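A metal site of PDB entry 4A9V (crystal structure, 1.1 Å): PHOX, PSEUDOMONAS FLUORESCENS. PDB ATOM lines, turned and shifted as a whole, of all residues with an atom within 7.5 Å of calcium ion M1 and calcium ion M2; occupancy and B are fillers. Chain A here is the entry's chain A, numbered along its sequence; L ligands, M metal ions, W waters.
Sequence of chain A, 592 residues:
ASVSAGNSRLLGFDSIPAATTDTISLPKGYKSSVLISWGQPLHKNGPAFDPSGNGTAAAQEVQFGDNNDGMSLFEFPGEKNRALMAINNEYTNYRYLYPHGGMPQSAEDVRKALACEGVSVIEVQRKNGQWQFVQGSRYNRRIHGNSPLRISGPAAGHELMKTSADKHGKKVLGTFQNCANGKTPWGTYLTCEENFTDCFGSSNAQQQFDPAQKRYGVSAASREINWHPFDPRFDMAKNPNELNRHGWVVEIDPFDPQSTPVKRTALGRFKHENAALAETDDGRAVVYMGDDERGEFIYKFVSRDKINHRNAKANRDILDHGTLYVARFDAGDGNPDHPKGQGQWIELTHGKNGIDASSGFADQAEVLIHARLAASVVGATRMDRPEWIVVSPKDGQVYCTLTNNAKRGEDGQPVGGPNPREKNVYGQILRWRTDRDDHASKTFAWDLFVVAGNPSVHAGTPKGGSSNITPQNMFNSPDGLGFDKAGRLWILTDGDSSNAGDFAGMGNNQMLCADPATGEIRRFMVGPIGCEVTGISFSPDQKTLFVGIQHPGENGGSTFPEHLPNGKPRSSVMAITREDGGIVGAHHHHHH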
ATOM      1  N   ASP A  69     -32.179  21.726 -18.208  1.00  0.00           N
ATOM      2  CA  ASP A  69     -31.387  21.048 -19.221  1.00  0.00           C
ATOM      3  C   ASP A  69     -32.298  20.804 -20.449  1.00  0.00           C
ATOM      4  O   ASP A  69     -32.926  21.726 -20.954  1.00  0.00           O
ATOM      5  CB  ASP A  69     -30.761  19.787 -18.606  1.00  0.00           C
ATOM      6  CG  ASP A  69     -29.493  19.342 -19.298  1.00  0.00           C
ATOM      7  OD1 ASP A  69     -29.352  19.604 -20.521  1.00  0.00           O
ATOM      8  OD2 ASP A  69     -28.652  18.698 -18.621  1.00  0.00           O
ATOM      9  N   GLY A  70     -32.419  19.563 -20.907  1.00  0.00           N
ATOM     10  CA  GLY A  70     -33.247  19.305 -22.091  1.00  0.00           C
ATOM     11  C   GLY A  70     -34.705  19.640 -21.838  1.00  0.00           C
ATOM     12  O   GLY A  70     -35.199  19.551 -20.718  1.00  0.00           O
ATOM     13  N   GLU A  90     -31.394  18.753 -14.064  1.00  0.00           N
ATOM     14  CA  GLU A  90     -30.387  17.681 -14.083  1.00  0.00           C
ATOM     15  C   GLU A  90     -29.730  17.442 -12.727  1.00  0.00           C
ATOM     16  O   GLU A  90     -29.522  16.291 -12.334  1.00  0.00           O
ATOM     17  CB  GLU A  90     -29.325  17.966 -15.143  1.00  0.00           C
ATOM     18  CG  GLU A  90     -28.421  16.764 -15.376  1.00  0.00           C
ATOM     19  CD  GLU A  90     -27.303  17.020 -16.360  1.00  0.00           C
ATOM     20  OE1 GLU A  90     -26.670  18.088 -16.266  1.00  0.00           O
ATOM     21  OE2 GLU A  90     -27.016  16.110 -17.176  1.00  0.00           O
ATOM     22  N   CYS A 179     -30.945  14.588 -17.995  1.00  0.00           N
ATOM     23  CA  CYS A 179     -30.062  15.311 -18.886  1.00  0.00           C
ATOM     24  C   CYS A 179     -30.886  15.914 -20.017  1.00  0.00           C
ATOM     25  O   CYS A 179     -31.406  17.012 -19.889  1.00  0.00           O
ATOM     26  CB  CYS A 179     -28.971  14.360 -19.377  1.00  0.00           C
ATOM     27  SG  CYS A 179     -27.766  15.113 -20.461  1.00  0.00           S
ATOM     28  N   ALA A 180     -31.104  15.162 -21.096  1.00  0.00           N
ATOM     29  CA  ALA A 180     -31.915  15.702 -22.178  1.00  0.00           C
ATOM     30  C   ALA A 180     -33.093  14.776 -22.523  1.00  0.00           C
ATOM     31  O   ALA A 180     -33.609  14.066 -21.646  1.00  0.00           O
ATOM     32  CB  ALA A 180     -31.027  16.058 -23.382  1.00  0.00           C
ATOM     33  N   GLU A 194     -28.946  10.311 -16.936  1.00  0.00           N
ATOM     34  CA  GLU A 194     -27.560  10.267 -17.423  1.00  0.00           C
ATOM     35  C   GLU A 194     -26.605   9.869 -16.296  1.00  0.00           C
ATOM     36  O   GLU A 194     -26.395   8.684 -16.069  1.00  0.00           O
ATOM     37  CB  GLU A 194     -27.175  11.604 -18.081  1.00  0.00           C
ATOM     38  CG  GLU A 194     -25.770  11.603 -18.686  1.00  0.00           C
ATOM     39  CD  GLU A 194     -25.279  12.980 -19.055  1.00  0.00           C
ATOM     40  OE1 GLU A 194     -25.687  13.959 -18.386  1.00  0.00           O
ATOM     41  OE2 GLU A 194     -24.420  13.072 -19.953  1.00  0.00           O
ATOM     42  N   GLU A 273     -28.177  10.518 -22.754  1.00  0.00           N
ATOM     43  CA  GLU A 273     -28.193  11.966 -22.984  1.00  0.00           C
ATOM     44  C   GLU A 273     -29.576  12.411 -23.466  1.00  0.00           C
ATOM     45  O   GLU A 273     -30.335  13.027 -22.722  1.00  0.00           O
ATOM     46  CB  GLU A 273     -27.110  12.398 -23.949  1.00  0.00           C
ATOM     47  CG  GLU A 273     -27.045  13.912 -24.117  1.00  0.00           C
ATOM     48  CD  GLU A 273     -26.052  14.579 -23.191  1.00  0.00           C
ATOM     49  OE1 GLU A 273     -25.192  13.857 -22.624  1.00  0.00           O
ATOM     50  OE2 GLU A 273     -26.116  15.829 -23.073  1.00  0.00           O
ATOM     51  N   ASP A 292     -23.384   9.074 -22.752  1.00  0.00           N
ATOM     52  CA  ASP A 292     -22.330  10.062 -22.597  1.00  0.00           C
ATOM     53  C   ASP A 292     -21.301   9.630 -21.562  1.00  0.00           C
ATOM     54  O   ASP A 292     -21.371   9.982 -20.381  1.00  0.00           O
ATOM     55  CB  ASP A 292     -22.891  11.443 -22.266  1.00  0.00           C
ATOM     56  CG  ASP A 292     -21.797  12.472 -22.071  1.00  0.00           C
ATOM     57  OD1 ASP A 292     -20.620  12.149 -22.362  1.00  0.00           O
ATOM     58  OD2 ASP A 292     -22.104  13.599 -21.638  1.00  0.00           O
ATOM     59  N   ARG A 385     -17.650  10.446 -26.350  1.00  0.00           N
ATOM     60  CA  ARG A 385     -18.723  11.068 -25.564  1.00  0.00           C
ATOM     61  C   ARG A 385     -19.894  11.543 -26.413  1.00  0.00           C
ATOM     62  O   ARG A 385     -20.151  12.743 -26.549  1.00  0.00           O
ATOM     63  CB  ARG A 385     -18.201  12.216 -24.721  1.00  0.00           C
ATOM     64  CG  ARG A 385     -17.223  11.797 -23.649  1.00  0.00           C
ATOM     65  CD  ARG A 385     -16.902  12.956 -22.740  1.00  0.00           C
ATOM     66  NE  ARG A 385     -18.109  13.413 -22.066  1.00  0.00           N
ATOM     67  CZ  ARG A 385     -18.284  14.647 -21.607  1.00  0.00           C
ATOM     68  NH1 ARG A 385     -17.239  15.450 -21.477  1.00  0.00           N
ATOM     69  NH2 ARG A 385     -19.469  15.011 -21.136  1.00  0.00           N
ATOM     70  N   GLU A 387     -23.287  12.917 -27.068  1.00  0.00           N
ATOM     71  CA  GLU A 387     -24.316  13.659 -26.353  1.00  0.00           C
ATOM     72  C   GLU A 387     -25.579  13.720 -27.222  1.00  0.00           C
ATOM     73  O   GLU A 387     -26.145  12.664 -27.510  1.00  0.00           O
ATOM     74  CB  GLU A 387     -23.784  14.984 -25.793  1.00  0.00           C
ATOM     75  CG  GLU A 387     -22.799  14.737 -24.657  1.00  0.00           C
ATOM     76  CD  GLU A 387     -22.532  15.945 -23.785  1.00  0.00           C
ATOM     77  OE1 GLU A 387     -21.732  16.802 -24.217  1.00  0.00           O
ATOM     78  OE2 GLU A 387     -23.084  16.043 -22.659  1.00  0.00           O
ATOM     79  N   TRP A 388     -26.063  14.899 -27.603  1.00  0.00           N
ATOM     80  CA  TRP A 388     -27.380  14.952 -28.235  1.00  0.00           C
ATOM     81  C   TRP A 388     -27.375  14.424 -29.655  1.00  0.00           C
ATOM     82  O   TRP A 388     -26.435  14.646 -30.421  1.00  0.00           O
ATOM     83  CB  TRP A 388     -27.924  16.366 -28.255  1.00  0.00           C
ATOM     84  CG  TRP A 388     -28.293  16.921 -26.916  1.00  0.00           C
ATOM     85  CD1 TRP A 388     -27.527  16.934 -25.757  1.00  0.00           C
ATOM     86  CD2 TRP A 388     -29.414  17.800 -26.643  1.00  0.00           C
ATOM     87  NE1 TRP A 388     -28.114  17.729 -24.807  1.00  0.00           N
ATOM     88  CE2 TRP A 388     -29.223  18.311 -25.301  1.00  0.00           C
ATOM     89  CE3 TRP A 388     -30.476  18.281 -27.402  1.00  0.00           C
ATOM     90  CZ2 TRP A 388     -30.090  19.231 -24.736  1.00  0.00           C
ATOM     91  CZ3 TRP A 388     -31.326  19.228 -26.831  1.00  0.00           C
ATOM     92  CH2 TRP A 388     -31.132  19.696 -25.528  1.00  0.00           C
ATOM     93  N   THR A 401     -23.550  14.929 -31.463  1.00  0.00           N
ATOM     94  CA  THR A 401     -22.333  15.527 -30.945  1.00  0.00           C
ATOM     95  C   THR A 401     -21.474  14.464 -30.267  1.00  0.00           C
ATOM     96  O   THR A 401     -21.979  13.549 -29.601  1.00  0.00           O
ATOM     97  CB  THR A 401     -22.638  16.685 -29.977  1.00  0.00           C
ATOM     98  OG1 THR A 401     -23.514  16.212 -28.960  1.00  0.00           O
ATOM     99  CG2 THR A 401     -23.257  17.860 -30.703  1.00  0.00           C
ATOM    100  N   THR A 403     -18.619  15.085 -27.814  1.00  0.00           N
ATOM    101  CA  THR A 403     -18.322  16.384 -27.249  1.00  0.00           C
ATOM    102  C   THR A 403     -16.811  16.608 -27.062  1.00  0.00           C
ATOM    103  O   THR A 403     -16.320  17.719 -27.249  1.00  0.00           O
ATOM    104  CB  THR A 403     -19.148  16.659 -25.970  1.00  0.00           C
ATOM    105  OG1 THR A 403     -19.111  18.059 -25.696  1.00  0.00           O
ATOM    106  CG2 THR A 403     -18.641  15.893 -24.772  1.00  0.00           C
ATOM    107  N   ASN A 404     -16.109  15.547 -26.658  1.00  0.00           N
ATOM    108  CA  ASN A 404     -14.647  15.532 -26.529  1.00  0.00           C
ATOM    109  C   ASN A 404     -14.261  14.153 -25.987  1.00  0.00           C
ATOM    110  O   ASN A 404     -15.132  13.324 -25.682  1.00  0.00           O
ATOM    111  CB  ASN A 404     -14.141  16.660 -25.614  1.00  0.00           C
ATOM    112  CG  ASN A 404     -14.867  16.718 -24.284  1.00  0.00           C
ATOM    113  OD1 ASN A 404     -14.857  15.757 -23.509  1.00  0.00           O
ATOM    114  ND2 ASN A 404     -15.455  17.876 -23.979  1.00  0.00           N
ATOM    115  N   SER A 477     -16.527  21.667 -27.560  1.00  0.00           N
ATOM    116  CA  SER A 477     -17.419  20.781 -26.827  1.00  0.00           C
ATOM    117  C   SER A 477     -18.885  21.030 -27.171  1.00  0.00           C
ATOM    118  O   SER A 477     -19.721  21.266 -26.295  1.00  0.00           O
ATOM    119  CB  SER A 477     -17.188  20.922 -25.318  1.00  0.00           C
ATOM    120  OG  SER A 477     -15.827  20.682 -24.983  1.00  0.00           O
ATOM    121  N   PRO A 478     -19.236  20.880 -28.452  1.00  0.00           N
ATOM    122  CA  PRO A 478     -20.655  20.867 -28.795  1.00  0.00           C
ATOM    123  C   PRO A 478     -21.363  19.747 -28.035  1.00  0.00           C
ATOM    124  O   PRO A 478     -20.790  18.689 -27.800  1.00  0.00           O
ATOM    125  CB  PRO A 478     -20.652  20.615 -30.295  1.00  0.00           C
ATOM    126  CG  PRO A 478     -19.410  19.808 -30.521  1.00  0.00           C
ATOM    127  CD  PRO A 478     -18.407  20.361 -29.553  1.00  0.00           C
ATOM    128  N   ASP A 479     -22.614  19.997 -27.659  1.00  0.00           N
ATOM    129  CA  ASP A 479     -23.310  19.131 -26.719  1.00  0.00           C
ATOM    130  C   ASP A 479     -24.772  19.044 -27.168  1.00  0.00           C
ATOM    131  O   ASP A 479     -25.141  18.126 -27.911  1.00  0.00           O
ATOM    132  CB  ASP A 479     -23.108  19.673 -25.281  1.00  0.00           C
ATOM    133  CG  ASP A 479     -23.807  18.869 -24.196  1.00  0.00           C
ATOM    134  OD1 ASP A 479     -24.848  18.228 -24.461  1.00  0.00           O
ATOM    135  OD2 ASP A 479     -23.383  19.002 -23.022  1.00  0.00           O
ATOM    136  N   GLY A 480     -25.551  20.082 -26.903  1.00  0.00           N
ATOM    137  CA  GLY A 480     -26.925  20.111 -27.381  1.00  0.00           C
ATOM    138  C   GLY A 480     -27.022  20.383 -28.868  1.00  0.00           C
ATOM    139  O   GLY A 480     -26.175  21.054 -29.467  1.00  0.00           O
ATOM    140  N   THR A 493     -23.183  24.640 -26.699  1.00  0.00           N
ATOM    141  CA  THR A 493     -21.904  24.185 -26.168  1.00  0.00           C
ATOM    142  C   THR A 493     -21.840  24.045 -24.657  1.00  0.00           C
ATOM    143  O   THR A 493     -22.466  24.808 -23.907  1.00  0.00           O
ATOM    144  CB  THR A 493     -20.695  25.016 -26.659  1.00  0.00           C
ATOM    145  OG1 THR A 493     -20.605  26.280 -25.980  1.00  0.00           O
ATOM    146  CG2 THR A 493     -20.765  25.256 -28.142  1.00  0.00           C
ATOM    147  N   ASP A 494     -21.054  23.063 -24.229  1.00  0.00           N
ATOM    148  CA  ASP A 494     -20.716  22.811 -22.836  1.00  0.00           C
ATOM    149  C   ASP A 494     -19.219  22.525 -22.741  1.00  0.00           C
ATOM    150  O   ASP A 494     -18.798  21.382 -22.583  1.00  0.00           O
ATOM    151  CB  ASP A 494     -21.507  21.625 -22.302  1.00  0.00           C
ATOM    152  CG  ASP A 494     -21.015  21.181 -20.947  1.00  0.00           C
ATOM    153  OD1 ASP A 494     -20.544  22.054 -20.187  1.00  0.00           O
ATOM    154  OD2 ASP A 494     -21.039  19.956 -20.667  1.00  0.00           O
ATOM    155  N   GLY A 495     -18.437  23.561 -22.971  1.00  0.00           N
ATOM    156  CA  GLY A 495     -17.000  23.410 -23.074  1.00  0.00           C
ATOM    157  C   GLY A 495     -16.242  24.236 -22.074  1.00  0.00           C
ATOM    158  O   GLY A 495     -16.810  24.828 -21.149  1.00  0.00           O
ATOM    159  N   GLU A 532     -23.382  26.506 -18.849  1.00  0.00           N
ATOM    160  CA  GLU A 532     -23.438  25.926 -20.189  1.00  0.00           C
ATOM    161  C   GLU A 532     -24.781  26.234 -20.817  1.00  0.00           C
ATOM    162  O   GLU A 532     -25.741  26.601 -20.140  1.00  0.00           O
ATOM    163  CB  GLU A 532     -23.167  24.414 -20.175  1.00  0.00           C
ATOM    164  CG  GLU A 532     -24.243  23.560 -19.523  1.00  0.00           C
ATOM    165  CD  GLU A 532     -23.778  22.117 -19.347  1.00  0.00           C
ATOM    166  OE1 GLU A 532     -23.075  21.850 -18.348  1.00  0.00           O
ATOM    167  OE2 GLU A 532     -24.121  21.258 -20.192  1.00  0.00           O
ATOM    168  N   VAL A 533     -24.804  26.217 -22.146  1.00  0.00           N
ATOM    169  CA  VAL A 533     -26.008  26.512 -22.916  1.00  0.00           C
ATOM    170  C   VAL A 533     -26.606  25.178 -23.325  1.00  0.00           C
ATOM    171  O   VAL A 533     -25.907  24.343 -23.911  1.00  0.00           O
ATOM    172  CB  VAL A 533     -25.637  27.355 -24.149  1.00  0.00           C
ATOM    173  CG1 VAL A 533     -26.847  27.561 -25.038  1.00  0.00           C
ATOM    174  CG2 VAL A 533     -25.063  28.700 -23.720  1.00  0.00           C
ATOM    175  N   THR A 534     -27.837  24.911 -22.910  1.00  0.00           N
ATOM    176  CA  THR A 534     -28.421  23.593 -23.044  1.00  0.00           C
ATOM    177  C   THR A 534     -29.932  23.705 -23.028  1.00  0.00           C
ATOM    178  O   THR A 534     -30.486  24.572 -22.360  1.00  0.00           O
ATOM    179  CB  THR A 534     -27.903  22.653 -21.958  1.00  0.00           C
ATOM    180  OG1 THR A 534     -28.311  21.315 -22.243  1.00  0.00           O
ATOM    181  CG2 THR A 534     -28.344  23.093 -20.572  1.00  0.00           C
ATOM    182  N   GLN A 550     -27.729  26.911 -17.963  1.00  0.00           N
ATOM    183  CA  GLN A 550     -27.594  25.971 -16.856  1.00  0.00           C
ATOM    184  C   GLN A 550     -26.377  26.320 -16.008  1.00  0.00           C
ATOM    185  O   GLN A 550     -25.313  26.637 -16.534  1.00  0.00           O
ATOM    186  CB  GLN A 550     -27.478  24.541 -17.400  1.00  0.00           C
ATOM    187  CG  GLN A 550     -27.633  23.468 -16.340  1.00  0.00           C
ATOM    188  CD  GLN A 550     -27.192  22.101 -16.815  1.00  0.00           C
ATOM    189  OE1 GLN A 550     -26.091  21.954 -17.351  1.00  0.00           O
ATOM    190  NE2 GLN A 550     -28.024  21.094 -16.597  1.00  0.00           N
HETATM  191 FE1  LIG L   1     -26.005  15.901 -18.946  1.00  0.00          FE
HETATM  192 FE2  LIG L   1     -23.838  14.535 -21.297  1.00  0.00          FE
HETATM  193  O1  LIG L   1     -24.677  16.005 -20.377  1.00  0.00           O
HETATM  194 CA    CA M   1     -21.606  18.009 -21.989  1.00  0.00          CA
HETATM  195 CA    CA M   2     -25.260  17.715 -22.039  1.00  0.00          CA
HETATM  196  O   HOH W   1     -19.727  18.847 -23.165  1.00  0.00           O
HETATM  197  O   HOH W   2     -26.292  17.988 -19.413  1.00  0.00           O
HETATM  198  O   HOH W   3     -23.487  18.592 -20.307  1.00  0.00           O
HETATM  199  O   HOH W   4     -25.823  20.138 -22.041  1.00  0.00           O
HETATM  200  O   HOH W   5     -27.762  17.905 -21.970  1.00  0.00           O
HETATM  201  O   HOH W   6     -21.419  17.002 -19.819  1.00  0.00           O
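Water W1 bridges OG1 of Thr 403 (2.7 Å) and O of Asp 494 (2.8 Å).
Water W2 bridges the side-chain carboxylate (OD2) of Asp 69 and the side-chain carboxylate (OE1) of Glu 90.
Water W5 lies within hydrogen-bond range of OD1 of Asp 69, NE1 of Trp 388 and OG1 of Thr 534.
Water W4 bridges the side-chain carboxylate (OE2) of Glu 532 (2.8 Å) and the side-chain hydroxyl (OG1) of Thr 534 (2.8 Å).
OE2 of Glu 273 binds calcium ion M2 (2.3 Å).
Calcium ion M2 is bound by O1 of the ligand, 2.5 Å away.
OD2 of Asp 479 is bound to calcium ion M2, 2.5 Å away.
Water W4 binds calcium ion M2 (2.5 Å).
Calcium ion M2 is bound by OD1 of Asp 479 (2.5 Å).
Water W5 binds calcium ion M2, 2.5 Å away.
Water W3 is bound to calcium ion M2 (2.6 Å).
OE2 of Glu 387 binds calcium ion M2 (2.8 Å).
Water W2 binds calcium ion M2, 2.8 Å away.
Calcium ion M1 is bound by the side-chain carboxylate (OD2) of Asp 479, 2.3 Å away.
Water W1 is bound to calcium ion M1.
Water W6 is bound to calcium ion M1.
Calcium ion M1 is bound by the side-chain carboxylate (OD2) of Asp 494, 2.4 Å away.
OE1 of Glu 387 binds calcium ion M1 (2.5 Å).
Calcium ion M1 is bound by OE2 of Glu 387, 2.5 Å away.
Water W3 is bound to calcium ion M1 (2.6 Å).
O of Arg 385 sits at hydrogen-bond distance from N of Thr 403, at 3.1 Å.
The backbone NH (N) of Glu 387 sits at hydrogen-bond distance from the backbone carbonyl oxygen (O) of Thr 401 (2.9 Å).
The backbone NH (N) of Asp 494 lies within hydrogen-bond range of the backbone carbonyl oxygen (O) of Ser 477 (3.0 Å).
The backbone carbonyl oxygen (O) of Asp 479 lies within hydrogen-bond range of the side-chain hydroxyl (OG1) of Thr 401.
The backbone NH (N) of Gly 70 sits at hydrogen-bond distance from the backbone carbonyl oxygen (O) of Cys 179 (2.9 Å).
NH1 of Arg 385 is in hydrogen-bond range of OD1 of Asn 404 (3.1 Å).
The backbone NH (N) of Trp 388 sits close to the backbone carbonyl oxygen (O) of Asp 479, 3.4 Å away.
The backbone NH of Ala 180 is in hydrogen-bond range of the backbone carbonyl oxygen of Glu 273, 2.8 Å away.
Merely in contact with calcium ion M1: Arg 385 (3.8 Å).
The nearest printed residue that does not touch calcium ion M1 is Asp 292 (4.5 Å).
An iron atom (FE2) of the ligand is bound by the side-chain carboxylate (OE2) of Glu 387, 2.2 Å away.
FE1 of the ligand is bound by OE2 of Glu 90 (2.0 Å).
SG of Cys 179 is bound to FE1 of the ligand (2.5 Å).
FE1 of the ligand is bound by OE1 of Glu 194 (2.0 Å).
OE1 of Glu 273 binds FE2 of the ligand (2.0 Å).
FE2 of the ligand is bound by OD2 of Asp 292, 2.0 Å away.
Residues that only touch calcium ion M2: Cys 179 and Trp 388.
Within 4 Å of calcium ion M2: Cys 179, Glu 273, Glu 387, Trp 388 and Asp 479.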
